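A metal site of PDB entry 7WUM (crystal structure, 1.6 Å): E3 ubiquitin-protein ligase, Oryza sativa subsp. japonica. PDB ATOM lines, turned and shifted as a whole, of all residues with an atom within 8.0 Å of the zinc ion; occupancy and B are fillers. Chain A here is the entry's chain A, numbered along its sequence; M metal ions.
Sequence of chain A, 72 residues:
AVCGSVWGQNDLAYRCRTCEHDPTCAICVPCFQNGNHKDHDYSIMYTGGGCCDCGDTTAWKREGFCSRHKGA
O of Cys 19 is in hydrogen-bond range of N of Lys 61 (2.8 Å).
A ring nitrogen (NE2) of His 37 lies close to the backbone carbonyl oxygen (O) of Gly 64.
SG of Cys 16 sits close to N of Thr 18 (3.6 Å).
Within 4 Å of the zinc ion: Cys 16, Cys 19, His 37 and His 40.
The nearest printed residue that does not touch the zinc ion is Thr 18 (4.2 Å).
The zinc ion is bound by a ring nitrogen (ND1) of His 37, a ring nitrogen (ND1) of His 40, the side-chain sulfur of Cys 16 and the side-chain sulfur of Cys 19.
The zinc ion has four donor atoms within binding distance.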
ATOM      1  N   ARG A  15       0.083 -20.663  23.481  1.00  0.00           N
ATOM      2  CA  ARG A  15      -0.347 -21.335  24.683  1.00  0.00           C
ATOM      3  C   ARG A  15       0.825 -21.377  25.645  1.00  0.00           C
ATOM      4  O   ARG A  15       1.973 -21.507  25.222  1.00  0.00           O
ATOM      5  CB  ARG A  15      -0.747 -22.784  24.424  1.00  0.00           C
ATOM      6  CG  ARG A  15      -1.783 -23.061  23.378  1.00  0.00           C
ATOM      7  CD  ARG A  15      -3.158 -22.717  23.790  1.00  0.00           C
ATOM      8  NE  ARG A  15      -4.104 -23.353  22.876  1.00  0.00           N
ATOM      9  CZ  ARG A  15      -5.399 -23.080  22.853  1.00  0.00           C
ATOM     10  NH1 ARG A  15      -5.926 -22.205  23.696  1.00  0.00           N
ATOM     11  NH2 ARG A  15      -6.176 -23.678  21.959  1.00  0.00           N
ATOM     12  N   CYS A  16       0.544 -21.295  26.933  1.00  0.00           N
ATOM     13  CA  CYS A  16       1.580 -21.543  27.931  1.00  0.00           C
ATOM     14  C   CYS A  16       0.955 -22.382  29.020  1.00  0.00           C
ATOM     15  O   CYS A  16       0.095 -21.915  29.762  1.00  0.00           O
ATOM     16  CB  CYS A  16       2.170 -20.259  28.502  1.00  0.00           C
ATOM     17  SG  CYS A  16       3.610 -20.679  29.536  1.00  0.00           S
ATOM     18  N   ARG A  17       1.342 -23.646  29.085  1.00  0.00           N
ATOM     19  CA  ARG A  17       0.806 -24.477  30.159  1.00  0.00           C
ATOM     20  C   ARG A  17       1.301 -24.129  31.601  1.00  0.00           C
ATOM     21  O   ARG A  17       0.698 -24.448  32.678  1.00  0.00           O
ATOM     22  CB  ARG A  17       1.107 -25.933  29.824  1.00  0.00           C
ATOM     23  CG  ARG A  17      -0.049 -26.587  29.110  1.00  0.00           C
ATOM     24  CD  ARG A  17      -0.029 -26.228  27.625  1.00  0.00           C
ATOM     25  NE  ARG A  17       1.299 -26.373  27.048  1.00  0.00           N
ATOM     26  CZ  ARG A  17       1.533 -26.478  25.749  1.00  0.00           C
ATOM     27  NH1 ARG A  17       0.547 -26.408  24.862  1.00  0.00           N
ATOM     28  NH2 ARG A  17       2.780 -26.673  25.313  1.00  0.00           N
ATOM     29  N   THR A  18       2.408 -23.381  31.630  1.00  0.00           N
ATOM     30  CA  THR A  18       2.864 -22.885  32.913  1.00  0.00           C
ATOM     31  C   THR A  18       1.990 -21.754  33.425  1.00  0.00           C
ATOM     32  O   THR A  18       1.713 -21.666  34.632  1.00  0.00           O
ATOM     33  CB  THR A  18       4.312 -22.443  32.774  1.00  0.00           C
ATOM     34  OG1 THR A  18       5.070 -23.511  32.191  1.00  0.00           O
ATOM     35  CG2 THR A  18       4.891 -22.117  34.120  1.00  0.00           C
ATOM     36  N   CYS A  19       1.521 -20.876  32.532  1.00  0.00           N
ATOM     37  CA  CYS A  19       0.793 -19.684  32.934  1.00  0.00           C
ATOM     38  C   CYS A  19      -0.732 -19.799  32.893  1.00  0.00           C
ATOM     39  O   CYS A  19      -1.409 -19.007  33.561  1.00  0.00           O
ATOM     40  CB  CYS A  19       1.197 -18.503  32.061  1.00  0.00           C
ATOM     41  SG  CYS A  19       2.859 -17.938  32.363  1.00  0.00           S
ATOM     42  N   GLU A  20      -1.283 -20.746  32.123  1.00  0.00           N
ATOM     43  CA  GLU A  20      -2.720 -20.800  31.886  1.00  0.00           C
ATOM     44  C   GLU A  20      -3.487 -21.274  33.125  1.00  0.00           C
ATOM     45  O   GLU A  20      -2.977 -22.050  33.946  1.00  0.00           O
ATOM     46  CB  GLU A  20      -3.030 -21.761  30.734  1.00  0.00           C
ATOM     47  CG  GLU A  20      -2.850 -23.220  31.155  1.00  0.00           C
ATOM     48  CD  GLU A  20      -3.018 -24.234  30.032  1.00  0.00           C
ATOM     49  OE1 GLU A  20      -2.744 -23.900  28.859  1.00  0.00           O
ATOM     50  OE2 GLU A  20      -3.427 -25.381  30.331  1.00  0.00           O
ATOM     51  N   ILE A  27      -2.444 -16.321  24.643  1.00  0.00           N
ATOM     52  CA  ILE A  27      -2.082 -14.914  24.567  1.00  0.00           C
ATOM     53  C   ILE A  27      -1.509 -14.619  23.189  1.00  0.00           C
ATOM     54  O   ILE A  27      -0.961 -15.495  22.516  1.00  0.00           O
ATOM     55  CB  ILE A  27      -1.107 -14.483  25.694  1.00  0.00           C
ATOM     56  CG1 ILE A  27       0.245 -15.180  25.596  1.00  0.00           C
ATOM     57  CG2 ILE A  27      -1.781 -14.659  27.071  1.00  0.00           C
ATOM     58  CD1 ILE A  27       1.246 -14.667  26.613  1.00  0.00           C
ATOM     59  N   PHE A  32       3.193 -12.378  24.343  1.00  0.00           N
ATOM     60  CA  PHE A  32       4.172 -13.385  24.722  1.00  0.00           C
ATOM     61  C   PHE A  32       5.582 -12.835  24.631  1.00  0.00           C
ATOM     62  O   PHE A  32       6.402 -13.036  25.540  1.00  0.00           O
ATOM     63  CB  PHE A  32       4.024 -14.637  23.847  1.00  0.00           C
ATOM     64  CG  PHE A  32       4.995 -15.717  24.180  1.00  0.00           C
ATOM     65  CD1 PHE A  32       6.283 -15.700  23.650  1.00  0.00           C
ATOM     66  CD2 PHE A  32       4.640 -16.709  25.055  1.00  0.00           C
ATOM     67  CE1 PHE A  32       7.193 -16.730  23.992  1.00  0.00           C
ATOM     68  CE2 PHE A  32       5.540 -17.723  25.382  1.00  0.00           C
ATOM     69  CZ  PHE A  32       6.817 -17.710  24.868  1.00  0.00           C
ATOM     70  N   GLY A  35       6.649 -10.683  27.513  1.00  0.00           N
ATOM     71  CA  GLY A  35       6.604 -11.299  28.814  1.00  0.00           C
ATOM     72  C   GLY A  35       7.774 -12.249  29.026  1.00  0.00           C
ATOM     73  O   GLY A  35       8.661 -12.388  28.182  1.00  0.00           O
ATOM     74  N   ASN A  36       7.755 -12.907  30.177  1.00  0.00           N
ATOM     75  CA  ASN A  36       8.850 -13.740  30.658  1.00  0.00           C
ATOM     76  C   ASN A  36       8.339 -15.182  30.776  1.00  0.00           C
ATOM     77  O   ASN A  36       7.623 -15.508  31.719  1.00  0.00           O
ATOM     78  CB  ASN A  36       9.364 -13.224  31.994  1.00  0.00           C
ATOM     79  CG  ASN A  36       9.800 -11.771  31.915  1.00  0.00           C
ATOM     80  OD1 ASN A  36      10.500 -11.373  30.979  1.00  0.00           O
ATOM     81  ND2 ASN A  36       9.341 -10.955  32.872  1.00  0.00           N
ATOM     82  N   HIS A  37       8.684 -16.030  29.812  1.00  0.00           N
ATOM     83  CA  HIS A  37       8.254 -17.428  29.847  1.00  0.00           C
ATOM     84  C   HIS A  37       9.425 -18.372  29.674  1.00  0.00           C
ATOM     85  O   HIS A  37       9.248 -19.469  29.143  1.00  0.00           O
ATOM     86  CB  HIS A  37       7.208 -17.711  28.782  1.00  0.00           C
ATOM     87  CG  HIS A  37       6.008 -16.809  28.878  1.00  0.00           C
ATOM     88  ND1 HIS A  37       4.895 -17.137  29.628  1.00  0.00           N
ATOM     89  CD2 HIS A  37       5.787 -15.574  28.381  1.00  0.00           C
ATOM     90  CE1 HIS A  37       4.017 -16.139  29.553  1.00  0.00           C
ATOM     91  NE2 HIS A  37       4.538 -15.193  28.797  1.00  0.00           N
ATOM     92  N   LYS A  38      10.619 -17.967  30.078  1.00  0.00           N
ATOM     93  CA  LYS A  38      11.733 -18.881  29.924  1.00  0.00           C
ATOM     94  C   LYS A  38      11.622 -20.050  30.889  1.00  0.00           C
ATOM     95  O   LYS A  38      11.252 -19.897  32.064  1.00  0.00           O
ATOM     96  CB  LYS A  38      13.074 -18.148  30.049  1.00  0.00           C
ATOM     97  CG  LYS A  38      13.195 -16.986  29.077  1.00  0.00           C
ATOM     98  CD  LYS A  38      14.275 -16.002  29.480  1.00  0.00           C
ATOM     99  CE  LYS A  38      14.896 -15.351  28.274  1.00  0.00           C
ATOM    100  NZ  LYS A  38      15.961 -14.387  28.675  1.00  0.00           N
ATOM    101  N   ASP A  39      11.883 -21.241  30.348  1.00  0.00           N
ATOM    102  CA  ASP A  39      11.649 -22.539  30.953  1.00  0.00           C
ATOM    103  C   ASP A  39      10.178 -22.855  31.142  1.00  0.00           C
ATOM    104  O   ASP A  39       9.845 -23.854  31.776  1.00  0.00           O
ATOM    105  CB  ASP A  39      12.414 -22.690  32.296  1.00  0.00           C
ATOM    106  CG  ASP A  39      13.900 -23.087  32.098  1.00  0.00           C
ATOM    107  OD1 ASP A  39      14.285 -23.506  30.980  1.00  0.00           O
ATOM    108  OD2 ASP A  39      14.682 -22.980  33.077  1.00  0.00           O
ATOM    109  N   HIS A  40       9.265 -22.051  30.601  1.00  0.00           N
ATOM    110  CA  HIS A  40       7.867 -22.430  30.666  1.00  0.00           C
ATOM    111  C   HIS A  40       7.540 -23.460  29.584  1.00  0.00           C
ATOM    112  O   HIS A  40       8.230 -23.584  28.558  1.00  0.00           O
ATOM    113  CB  HIS A  40       6.953 -21.213  30.485  1.00  0.00           C
ATOM    114  CG  HIS A  40       7.020 -20.236  31.606  1.00  0.00           C
ATOM    115  ND1 HIS A  40       6.044 -19.297  31.829  1.00  0.00           N
ATOM    116  CD2 HIS A  40       7.944 -20.062  32.582  1.00  0.00           C
ATOM    117  CE1 HIS A  40       6.360 -18.583  32.893  1.00  0.00           C
ATOM    118  NE2 HIS A  40       7.508 -19.026  33.374  1.00  0.00           N
ATOM    119  N   ASP A  41       6.439 -24.188  29.805  1.00  0.00           N
ATOM    120  CA  ASP A  41       5.889 -25.127  28.831  1.00  0.00           C
ATOM    121  C   ASP A  41       4.974 -24.365  27.871  1.00  0.00           C
ATOM    122  O   ASP A  41       3.742 -24.420  27.957  1.00  0.00           O
ATOM    123  CB  ASP A  41       5.110 -26.234  29.520  1.00  0.00           C
ATOM    124  CG  ASP A  41       4.513 -27.251  28.535  1.00  0.00           C
ATOM    125  OD1 ASP A  41       4.980 -27.312  27.382  1.00  0.00           O
ATOM    126  OD2 ASP A  41       3.560 -27.963  28.926  1.00  0.00           O
ATOM    127  N   TYR A  42       5.579 -23.681  26.915  1.00  0.00           N
ATOM    128  CA  TYR A  42       4.814 -22.869  25.976  1.00  0.00           C
ATOM    129  C   TYR A  42       4.983 -23.389  24.566  1.00  0.00           C
ATOM    130  O   TYR A  42       5.982 -24.015  24.237  1.00  0.00           O
ATOM    131  CB  TYR A  42       5.250 -21.406  26.033  1.00  0.00           C
ATOM    132  CG  TYR A  42       6.661 -21.150  25.551  1.00  0.00           C
ATOM    133  CD1 TYR A  42       6.951 -21.010  24.187  1.00  0.00           C
ATOM    134  CD2 TYR A  42       7.705 -20.980  26.444  1.00  0.00           C
ATOM    135  CE1 TYR A  42       8.225 -20.750  23.739  1.00  0.00           C
ATOM    136  CE2 TYR A  42       8.980 -20.696  26.015  1.00  0.00           C
ATOM    137  CZ  TYR A  42       9.240 -20.592  24.661  1.00  0.00           C
ATOM    138  OH  TYR A  42      10.521 -20.327  24.219  1.00  0.00           O
ATOM    139  N   TRP A  60      -5.119 -16.186  33.373  1.00  0.00           N
ATOM    140  CA  TRP A  60      -3.689 -16.256  33.166  1.00  0.00           C
ATOM    141  C   TRP A  60      -2.983 -15.809  34.440  1.00  0.00           C
ATOM    142  O   TRP A  60      -3.367 -14.806  35.040  1.00  0.00           O
ATOM    143  CB  TRP A  60      -3.318 -15.356  31.991  1.00  0.00           C
ATOM    144  CG  TRP A  60      -2.029 -15.639  31.273  1.00  0.00           C
ATOM    145  CD1 TRP A  60      -0.840 -14.988  31.440  1.00  0.00           C
ATOM    146  CD2 TRP A  60      -1.831 -16.565  30.198  1.00  0.00           C
ATOM    147  NE1 TRP A  60       0.101 -15.480  30.573  1.00  0.00           N
ATOM    148  CE2 TRP A  60      -0.484 -16.445  29.789  1.00  0.00           C
ATOM    149  CE3 TRP A  60      -2.652 -17.498  29.561  1.00  0.00           C
ATOM    150  CZ2 TRP A  60       0.060 -17.213  28.776  1.00  0.00           C
ATOM    151  CZ3 TRP A  60      -2.108 -18.266  28.548  1.00  0.00           C
ATOM    152  CH2 TRP A  60      -0.778 -18.119  28.159  1.00  0.00           C
ATOM    153  N   LYS A  61      -1.947 -16.555  34.830  1.00  0.00           N
ATOM    154  CA  LYS A  61      -1.199 -16.214  36.033  1.00  0.00           C
ATOM    155  C   LYS A  61      -0.503 -14.865  35.878  1.00  0.00           C
ATOM    156  O   LYS A  61       0.000 -14.515  34.806  1.00  0.00           O
ATOM    157  CB  LYS A  61      -0.190 -17.323  36.335  1.00  0.00           C
ATOM    158  CG  LYS A  61      -0.843 -18.566  36.915  1.00  0.00           C
ATOM    159  CD  LYS A  61       0.121 -19.747  36.967  1.00  0.00           C
ATOM    160  CE  LYS A  61      -0.589 -21.085  36.754  1.00  0.00           C
ATOM    161  NZ  LYS A  61       0.331 -22.240  36.989  1.00  0.00           N
ATOM    162  N   GLU A  63       2.277 -13.682  36.826  1.00  0.00           N
ATOM    163  CA  GLU A  63       3.692 -13.713  36.486  1.00  0.00           C
ATOM    164  C   GLU A  63       3.905 -13.852  34.985  1.00  0.00           C
ATOM    165  O   GLU A  63       4.995 -13.560  34.489  1.00  0.00           O
ATOM    166  CB  GLU A  63       4.385 -14.863  37.217  1.00  0.00           C
ATOM    167  CG  GLU A  63       3.989 -15.000  38.684  1.00  0.00           C
ATOM    168  CD  GLU A  63       2.608 -15.642  38.855  1.00  0.00           C
ATOM    169  OE1 GLU A  63       1.598 -14.896  38.916  1.00  0.00           O
ATOM    170  OE2 GLU A  63       2.538 -16.888  38.936  1.00  0.00           O
ATOM    171  N   GLY A  64       2.883 -14.289  34.249  1.00  0.00           N
ATOM    172  CA  GLY A  64       2.930 -14.446  32.820  1.00  0.00           C
ATOM    173  C   GLY A  64       2.380 -13.288  32.037  1.00  0.00           C
ATOM    174  O   GLY A  64       2.380 -13.354  30.804  1.00  0.00           O
ATOM    175  N   PHE A  65       1.927 -12.224  32.704  1.00  0.00           N
ATOM    176  CA  PHE A  65       1.487 -11.032  31.986  1.00  0.00           C
ATOM    177  C   PHE A  65       2.678 -10.336  31.345  1.00  0.00           C
ATOM    178  O   PHE A  65       3.772 -10.277  31.907  1.00  0.00           O
ATOM    179  CB  PHE A  65       0.812 -10.031  32.920  1.00  0.00           C
ATOM    180  CG  PHE A  65      -0.480 -10.499  33.537  1.00  0.00           C
ATOM    181  CD1 PHE A  65      -1.112 -11.659  33.113  1.00  0.00           C
ATOM    182  CD2 PHE A  65      -1.092  -9.730  34.531  1.00  0.00           C
ATOM    183  CE1 PHE A  65      -2.309 -12.063  33.685  1.00  0.00           C
ATOM    184  CE2 PHE A  65      -2.282 -10.130  35.109  1.00  0.00           C
ATOM    185  CZ  PHE A  65      -2.890 -11.301  34.697  1.00  0.00           C
HETATM  186 ZN    ZN M   1       4.298 -18.826  30.734  1.00  0.00          ZN
